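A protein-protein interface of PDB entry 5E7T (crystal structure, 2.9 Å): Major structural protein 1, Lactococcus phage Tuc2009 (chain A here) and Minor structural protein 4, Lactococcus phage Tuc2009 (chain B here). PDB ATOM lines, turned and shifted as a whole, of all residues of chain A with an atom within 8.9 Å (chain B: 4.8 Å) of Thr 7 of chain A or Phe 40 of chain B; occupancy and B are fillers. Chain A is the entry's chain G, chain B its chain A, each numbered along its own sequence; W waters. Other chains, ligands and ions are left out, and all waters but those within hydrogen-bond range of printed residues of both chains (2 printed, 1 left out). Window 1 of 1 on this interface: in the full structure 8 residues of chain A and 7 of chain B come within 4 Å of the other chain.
The guanidinium group of Arg 8 of chain A sits at hydrogen-bond distance from the backbone carbonyl oxygen of Gly 42 of chain B (3.2 Å).
OD2 of Asp 35 of chain B sits at hydrogen-bond distance from N of Gly 13 of chain A (3.3 Å).
The backbone carbonyl oxygen of Gly 41 of chain B is in hydrogen-bond range of the guanidinium group of Arg 8 of chain A (3.0 Å).
O of Phe 40 of chain B lies within hydrogen-bond range of N of Gly 9 of chain A.
The side-chain carboxylate (OD2) of Asp 35 of chain B lies within hydrogen-bond range of the backbone NH (N) of Ala 14 of chain A, 2.8 Å away.
The backbone NH of Thr 7 of chain A sits at hydrogen-bond distance from the side-chain sulfur of Met 10 of chain A (3.6 Å).
Among the printed residues, merely in contact across the chains: Ile 6 of chain A with Phe 40 of chain B (3.9 Å), Thr 7 of chain A with Phe 40 of chain B (3.8 Å), Arg 8 of chain A with Phe 40 of chain B (3.4 Å), Gly 9 of chain A with Val 39 of chain B (3.7 Å), Met 10 of chain A with Phe 40 of chain B (3.7 Å), Ile 17 of chain A with Phe 34 of chain B (3.97 Å) and Ile 17 of chain A with Phe 40 of chain B (3.5 Å).
Of chain B, only Phe 40 comes within 4 Å of Thr 7 of chain A.
Of the printed residues of chain B, Met 10 of chain A touches Phe 40.
Of the printed residues of chain A, Phe 34 of chain B touches Ile 17 (3.97 Å).
Printed residues of chain A within 4 Å of Asp 35 of chain B: Gly 13 and Ala 14.
Of the printed residues of chain A, Val 39 of chain B touches Gly 9 (3.7 Å).
Phe 40 of chain B touches six residues of chain A.
Of chain A, only Arg 8 (3.0 Å) comes within 4 Å of Gly 41 of chain B.
The nearest residue of chain A that does not touch Phe 40 of chain B is Gly 13 of chain A (4.6 Å).
The nearest printed residue of chain B that does not touch Met 10 of chain A is Asp 35 of chain B (4.9 Å).
Of the 15 printed residues of chain A, 8 touch a printed residue of chain B.
Hydrophobic or aromatic side chains of chain A within 4 Å of the printed part of chain B: Ile 6, Ala 14 and Ile 17.
Hydrophobic or aromatic side chains of chain B within 4 Å of the printed part of chain A: Phe 34, Val 39 and Phe 40.
Among the printed residues, 12 pairs touch across the chains.
Among the printed residues, no Asp or Glu carboxylate lies within 4 Å of a Lys or Arg side-chain nitrogen of the other chain.
Water W2 lies within hydrogen-bond range of the backbone carbonyl oxygen (O) of Met 10 of chain A, the backbone NH (N) of Gly 13 of chain A, the side-chain carboxylate (OD1) of Asp 35 of chain B and the backbone NH (N) of Asn 12 of chain A.
Water W1 lies within hydrogen-bond range of the backbone carbonyl oxygen (O) of Gly 41 of chain B (2.9 Å) and the guanidinium group (NH1) of Arg 8 of chain A (2.9 Å).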
ATOM      1  N   THR A   4      15.847   5.469   4.387  1.00  0.00           N
ATOM      2  CA  THR A   4      15.503   5.136   5.769  1.00  0.00           C
ATOM      3  C   THR A   4      16.317   3.901   6.195  1.00  0.00           C
ATOM      4  O   THR A   4      16.279   2.875   5.511  1.00  0.00           O
ATOM      5  CB  THR A   4      13.976   4.974   5.911  1.00  0.00           C
ATOM      6  OG1 THR A   4      13.307   6.165   5.491  1.00  0.00           O
ATOM      7  CG2 THR A   4      13.559   4.631   7.286  1.00  0.00           C
ATOM      8  N   LYS A   5      17.067   4.011   7.311  1.00  0.00           N
ATOM      9  CA  LYS A   5      17.931   2.948   7.827  1.00  0.00           C
ATOM     10  C   LYS A   5      17.199   1.637   8.085  1.00  0.00           C
ATOM     11  O   LYS A   5      16.118   1.635   8.685  1.00  0.00           O
ATOM     12  CB  LYS A   5      18.645   3.420   9.097  1.00  0.00           C
ATOM     13  CG  LYS A   5      19.880   2.614   9.470  1.00  0.00           C
ATOM     14  CD  LYS A   5      20.453   3.078  10.789  1.00  0.00           C
ATOM     15  CE  LYS A   5      21.644   2.258  11.206  1.00  0.00           C
ATOM     16  NZ  LYS A   5      22.596   3.055  12.040  1.00  0.00           N
ATOM     17  N   ILE A   6      17.804   0.529   7.613  1.00  0.00           N
ATOM     18  CA  ILE A   6      17.340  -0.855   7.781  1.00  0.00           C
ATOM     19  C   ILE A   6      18.147  -1.430   8.938  1.00  0.00           C
ATOM     20  O   ILE A   6      19.368  -1.581   8.820  1.00  0.00           O
ATOM     21  CB  ILE A   6      17.516  -1.697   6.478  1.00  0.00           C
ATOM     22  CG1 ILE A   6      16.802  -1.050   5.263  1.00  0.00           C
ATOM     23  CG2 ILE A   6      17.091  -3.148   6.675  1.00  0.00           C
ATOM     24  CD1 ILE A   6      15.341  -0.740   5.443  1.00  0.00           C
ATOM     25  N   THR A   7      17.474  -1.717  10.060  1.00  0.00           N
ATOM     26  CA  THR A   7      18.107  -2.257  11.253  1.00  0.00           C
ATOM     27  C   THR A   7      17.510  -3.604  11.681  1.00  0.00           C
ATOM     28  O   THR A   7      16.358  -3.899  11.373  1.00  0.00           O
ATOM     29  CB  THR A   7      18.017  -1.246  12.400  1.00  0.00           C
ATOM     30  OG1 THR A   7      16.647  -0.998  12.728  1.00  0.00           O
ATOM     31  CG2 THR A   7      18.750   0.034  12.104  1.00  0.00           C
ATOM     32  N   ARG A   8      18.285  -4.395  12.447  1.00  0.00           N
ATOM     33  CA  ARG A   8      17.832  -5.660  13.035  1.00  0.00           C
ATOM     34  C   ARG A   8      16.726  -5.342  14.037  1.00  0.00           C
ATOM     35  O   ARG A   8      16.867  -4.448  14.864  1.00  0.00           O
ATOM     36  CB  ARG A   8      19.013  -6.308  13.772  1.00  0.00           C
ATOM     37  CG  ARG A   8      18.777  -7.665  14.374  1.00  0.00           C
ATOM     38  CD  ARG A   8      20.100  -8.270  14.799  1.00  0.00           C
ATOM     39  NE  ARG A   8      20.190  -9.676  14.406  1.00  0.00           N
ATOM     40  CZ  ARG A   8      20.843 -10.126  13.337  1.00  0.00           C
ATOM     41  NH1 ARG A   8      21.525  -9.286  12.565  1.00  0.00           N
ATOM     42  NH2 ARG A   8      20.842 -11.420  13.047  1.00  0.00           N
ATOM     43  N   GLY A   9      15.624  -6.049  13.934  1.00  0.00           N
ATOM     44  CA  GLY A   9      14.500  -5.879  14.842  1.00  0.00           C
ATOM     45  C   GLY A   9      13.479  -4.826  14.463  1.00  0.00           C
ATOM     46  O   GLY A   9      12.466  -4.678  15.160  1.00  0.00           O
ATOM     47  N   MET A  10      13.744  -4.067  13.396  1.00  0.00           N
ATOM     48  CA  MET A  10      12.861  -2.999  12.960  1.00  0.00           C
ATOM     49  C   MET A  10      11.490  -3.506  12.575  1.00  0.00           C
ATOM     50  O   MET A  10      11.302  -4.678  12.185  1.00  0.00           O
ATOM     51  CB  MET A  10      13.476  -2.201  11.781  1.00  0.00           C
ATOM     52  CG  MET A  10      13.290  -2.855  10.414  1.00  0.00           C
ATOM     53  SD  MET A  10      13.997  -1.910   9.094  1.00  0.00           S
ATOM     54  CE  MET A  10      13.018  -0.485   9.140  1.00  0.00           C
ATOM     55  N   GLN A  11      10.549  -2.583  12.665  1.00  0.00           N
ATOM     56  CA  GLN A  11       9.184  -2.768  12.239  1.00  0.00           C
ATOM     57  C   GLN A  11       9.129  -2.188  10.851  1.00  0.00           C
ATOM     58  O   GLN A  11       9.824  -1.213  10.543  1.00  0.00           O
ATOM     59  CB  GLN A  11       8.209  -2.024  13.162  1.00  0.00           C
ATOM     60  CG  GLN A  11       8.036  -2.669  14.530  1.00  0.00           C
ATOM     61  CD  GLN A  11       7.630  -4.114  14.484  1.00  0.00           C
ATOM     62  OE1 GLN A  11       6.556  -4.478  13.994  1.00  0.00           O
ATOM     63  NE2 GLN A  11       8.494  -4.968  14.982  1.00  0.00           N
ATOM     64  N   ASN A  12       8.298  -2.787  10.022  1.00  0.00           N
ATOM     65  CA  ASN A  12       8.059  -2.391   8.642  1.00  0.00           C
ATOM     66  C   ASN A  12       9.277  -2.570   7.766  1.00  0.00           C
ATOM     67  O   ASN A  12       9.511  -1.768   6.857  1.00  0.00           O
ATOM     68  CB  ASN A  12       7.495  -0.980   8.563  1.00  0.00           C
ATOM     69  CG  ASN A  12       6.281  -0.755   9.447  1.00  0.00           C
ATOM     70  OD1 ASN A  12       5.277  -1.504   9.405  1.00  0.00           O
ATOM     71  ND2 ASN A  12       6.347   0.313  10.231  1.00  0.00           N
ATOM     72  N   GLY A  13      10.012  -3.655   8.024  1.00  0.00           N
ATOM     73  CA  GLY A  13      11.231  -4.024   7.314  1.00  0.00           C
ATOM     74  C   GLY A  13      11.021  -4.184   5.828  1.00  0.00           C
ATOM     75  O   GLY A  13      11.736  -3.559   5.058  1.00  0.00           O
ATOM     76  N   ALA A  14      10.017  -4.992   5.412  1.00  0.00           N
ATOM     77  CA  ALA A  14       9.718  -5.257   4.016  1.00  0.00           C
ATOM     78  C   ALA A  14       9.366  -3.991   3.270  1.00  0.00           C
ATOM     79  O   ALA A  14       9.912  -3.743   2.194  1.00  0.00           O
ATOM     80  CB  ALA A  14       8.605  -6.271   3.892  1.00  0.00           C
ATOM     81  N   GLU A  15       8.514  -3.152   3.849  1.00  0.00           N
ATOM     82  CA  GLU A  15       8.094  -1.904   3.194  1.00  0.00           C
ATOM     83  C   GLU A  15       9.221  -0.903   3.127  1.00  0.00           C
ATOM     84  O   GLU A  15       9.382  -0.273   2.078  1.00  0.00           O
ATOM     85  CB  GLU A  15       6.877  -1.285   3.872  1.00  0.00           C
ATOM     86  CG  GLU A  15       5.724  -2.252   4.009  1.00  0.00           C
ATOM     87  CD  GLU A  15       5.673  -3.019   5.302  1.00  0.00           C
ATOM     88  OE1 GLU A  15       6.747  -3.306   5.876  1.00  0.00           O
ATOM     89  OE2 GLU A  15       4.548  -3.310   5.762  1.00  0.00           O
ATOM     90  N   THR A  16      10.028  -0.776   4.224  1.00  0.00           N
ATOM     91  CA  THR A  16      11.145   0.162   4.215  1.00  0.00           C
ATOM     92  C   THR A  16      12.171  -0.261   3.174  1.00  0.00           C
ATOM     93  O   THR A  16      12.659   0.603   2.447  1.00  0.00           O
ATOM     94  CB  THR A  16      11.710   0.383   5.612  1.00  0.00           C
ATOM     95  OG1 THR A  16      10.657   0.668   6.546  1.00  0.00           O
ATOM     96  CG2 THR A  16      12.676   1.506   5.652  1.00  0.00           C
ATOM     97  N   ILE A  17      12.442  -1.586   3.034  1.00  0.00           N
ATOM     98  CA  ILE A  17      13.366  -2.108   2.006  1.00  0.00           C
ATOM     99  C   ILE A  17      12.777  -1.777   0.617  1.00  0.00           C
ATOM    100  O   ILE A  17      13.489  -1.269  -0.256  1.00  0.00           O
ATOM    101  CB  ILE A  17      13.694  -3.620   2.174  1.00  0.00           C
ATOM    102  CG1 ILE A  17      14.464  -3.882   3.469  1.00  0.00           C
ATOM    103  CG2 ILE A  17      14.514  -4.142   0.984  1.00  0.00           C
ATOM    104  CD1 ILE A  17      14.444  -5.290   3.921  1.00  0.00           C
ATOM    105  N   ASN A  20      13.032   1.951  -0.144  1.00  0.00           N
ATOM    106  CA  ASN A  20      14.428   2.297  -0.406  1.00  0.00           C
ATOM    107  C   ASN A  20      14.901   1.851  -1.796  1.00  0.00           C
ATOM    108  O   ASN A  20      15.579   2.618  -2.488  1.00  0.00           O
ATOM    109  CB  ASN A  20      15.328   1.791   0.704  1.00  0.00           C
ATOM    110  CG  ASN A  20      15.119   2.495   2.024  1.00  0.00           C
ATOM    111  OD1 ASN A  20      14.474   3.543   2.144  1.00  0.00           O
ATOM    112  ND2 ASN A  20      15.662   1.935   3.056  1.00  0.00           N
ATOM    113  N   ILE B  27      16.663 -13.744   7.807  1.00  0.00           N
ATOM    114  CA  ILE B  27      15.922 -13.503   6.557  1.00  0.00           C
ATOM    115  C   ILE B  27      15.817 -14.764   5.703  1.00  0.00           C
ATOM    116  O   ILE B  27      16.829 -15.374   5.394  1.00  0.00           O
ATOM    117  CB  ILE B  27      16.429 -12.267   5.741  1.00  0.00           C
ATOM    118  CG1 ILE B  27      17.943 -12.290   5.466  1.00  0.00           C
ATOM    119  CG2 ILE B  27      16.008 -10.965   6.436  1.00  0.00           C
ATOM    120  CD1 ILE B  27      18.305 -11.844   4.132  1.00  0.00           C
ATOM    121  N   PHE B  34       8.882 -13.989   4.131  1.00  0.00           N
ATOM    122  CA  PHE B  34       9.795 -12.871   4.403  1.00  0.00           C
ATOM    123  C   PHE B  34       9.246 -11.858   5.368  1.00  0.00           C
ATOM    124  O   PHE B  34       8.174 -11.328   5.128  1.00  0.00           O
ATOM    125  CB  PHE B  34      10.233 -12.159   3.101  1.00  0.00           C
ATOM    126  CG  PHE B  34      11.243 -11.055   3.327  1.00  0.00           C
ATOM    127  CD1 PHE B  34      12.585 -11.354   3.573  1.00  0.00           C
ATOM    128  CD2 PHE B  34      10.857  -9.719   3.288  1.00  0.00           C
ATOM    129  CE1 PHE B  34      13.509 -10.339   3.799  1.00  0.00           C
ATOM    130  CE2 PHE B  34      11.786  -8.705   3.496  1.00  0.00           C
ATOM    131  CZ  PHE B  34      13.100  -9.022   3.772  1.00  0.00           C
ATOM    132  N   ASP B  35      10.017 -11.551   6.427  1.00  0.00           N
ATOM    133  CA  ASP B  35       9.698 -10.536   7.455  1.00  0.00           C
ATOM    134  C   ASP B  35       8.402 -10.807   8.196  1.00  0.00           C
ATOM    135  O   ASP B  35       7.681  -9.870   8.502  1.00  0.00           O
ATOM    136  CB  ASP B  35       9.711  -9.097   6.866  1.00  0.00           C
ATOM    137  CG  ASP B  35       9.682  -7.955   7.862  1.00  0.00           C
ATOM    138  OD1 ASP B  35      10.042  -8.185   9.057  1.00  0.00           O
ATOM    139  OD2 ASP B  35       9.300  -6.827   7.459  1.00  0.00           O
ATOM    140  N   PRO B  38       9.417 -12.339  14.613  1.00  0.00           N
ATOM    141  CA  PRO B  38       9.299 -11.357  15.689  1.00  0.00           C
ATOM    142  C   PRO B  38      10.436 -10.335  15.782  1.00  0.00           C
ATOM    143  O   PRO B  38      10.322  -9.340  16.526  1.00  0.00           O
ATOM    144  CB  PRO B  38       9.242 -12.248  16.930  1.00  0.00           C
ATOM    145  CG  PRO B  38      10.043 -13.393  16.600  1.00  0.00           C
ATOM    146  CD  PRO B  38       9.930 -13.621  15.128  1.00  0.00           C
ATOM    147  N   VAL B  39      11.565 -10.610  15.106  1.00  0.00           N
ATOM    148  CA  VAL B  39      12.746  -9.739  15.149  1.00  0.00           C
ATOM    149  C   VAL B  39      13.367  -9.782  13.750  1.00  0.00           C
ATOM    150  O   VAL B  39      14.162 -10.702  13.458  1.00  0.00           O
ATOM    151  CB  VAL B  39      13.773 -10.173  16.248  1.00  0.00           C
ATOM    152  CG1 VAL B  39      14.916  -9.174  16.364  1.00  0.00           C
ATOM    153  CG2 VAL B  39      13.115 -10.417  17.613  1.00  0.00           C
ATOM    154  N   PHE B  40      12.987  -8.817  12.867  1.00  0.00           N
ATOM    155  CA  PHE B  40      13.482  -8.809  11.484  1.00  0.00           C
ATOM    156  C   PHE B  40      14.969  -8.902  11.446  1.00  0.00           C
ATOM    157  O   PHE B  40      15.635  -8.129  12.105  1.00  0.00           O
ATOM    158  CB  PHE B  40      12.986  -7.575  10.684  1.00  0.00           C
ATOM    159  CG  PHE B  40      13.660  -7.387   9.346  1.00  0.00           C
ATOM    160  CD1 PHE B  40      13.264  -8.124   8.242  1.00  0.00           C
ATOM    161  CD2 PHE B  40      14.724  -6.512   9.205  1.00  0.00           C
ATOM    162  CE1 PHE B  40      13.928  -7.992   7.016  1.00  0.00           C
ATOM    163  CE2 PHE B  40      15.407  -6.396   7.984  1.00  0.00           C
ATOM    164  CZ  PHE B  40      15.000  -7.132   6.897  1.00  0.00           C
ATOM    165  N   GLY B  41      15.482  -9.843  10.683  1.00  0.00           N
ATOM    166  CA  GLY B  41      16.925 -10.005  10.505  1.00  0.00           C
ATOM    167  C   GLY B  41      17.492 -11.126  11.335  1.00  0.00           C
ATOM    168  O   GLY B  41      18.577 -11.615  11.044  1.00  0.00           O
ATOM    169  N   GLY B  42      16.756 -11.531  12.366  1.00  0.00           N
ATOM    170  CA  GLY B  42      17.164 -12.633  13.222  1.00  0.00           C
ATOM    171  C   GLY B  42      17.121 -12.320  14.695  1.00  0.00           C
ATOM    172  O   GLY B  42      17.453 -11.208  15.102  1.00  0.00           O
HETATM  173  O   HOH W   1      20.063  -9.347  10.057  1.00  0.00           O
HETATM  174  O   HOH W   2       9.761  -5.483  10.083  1.00  0.00           O
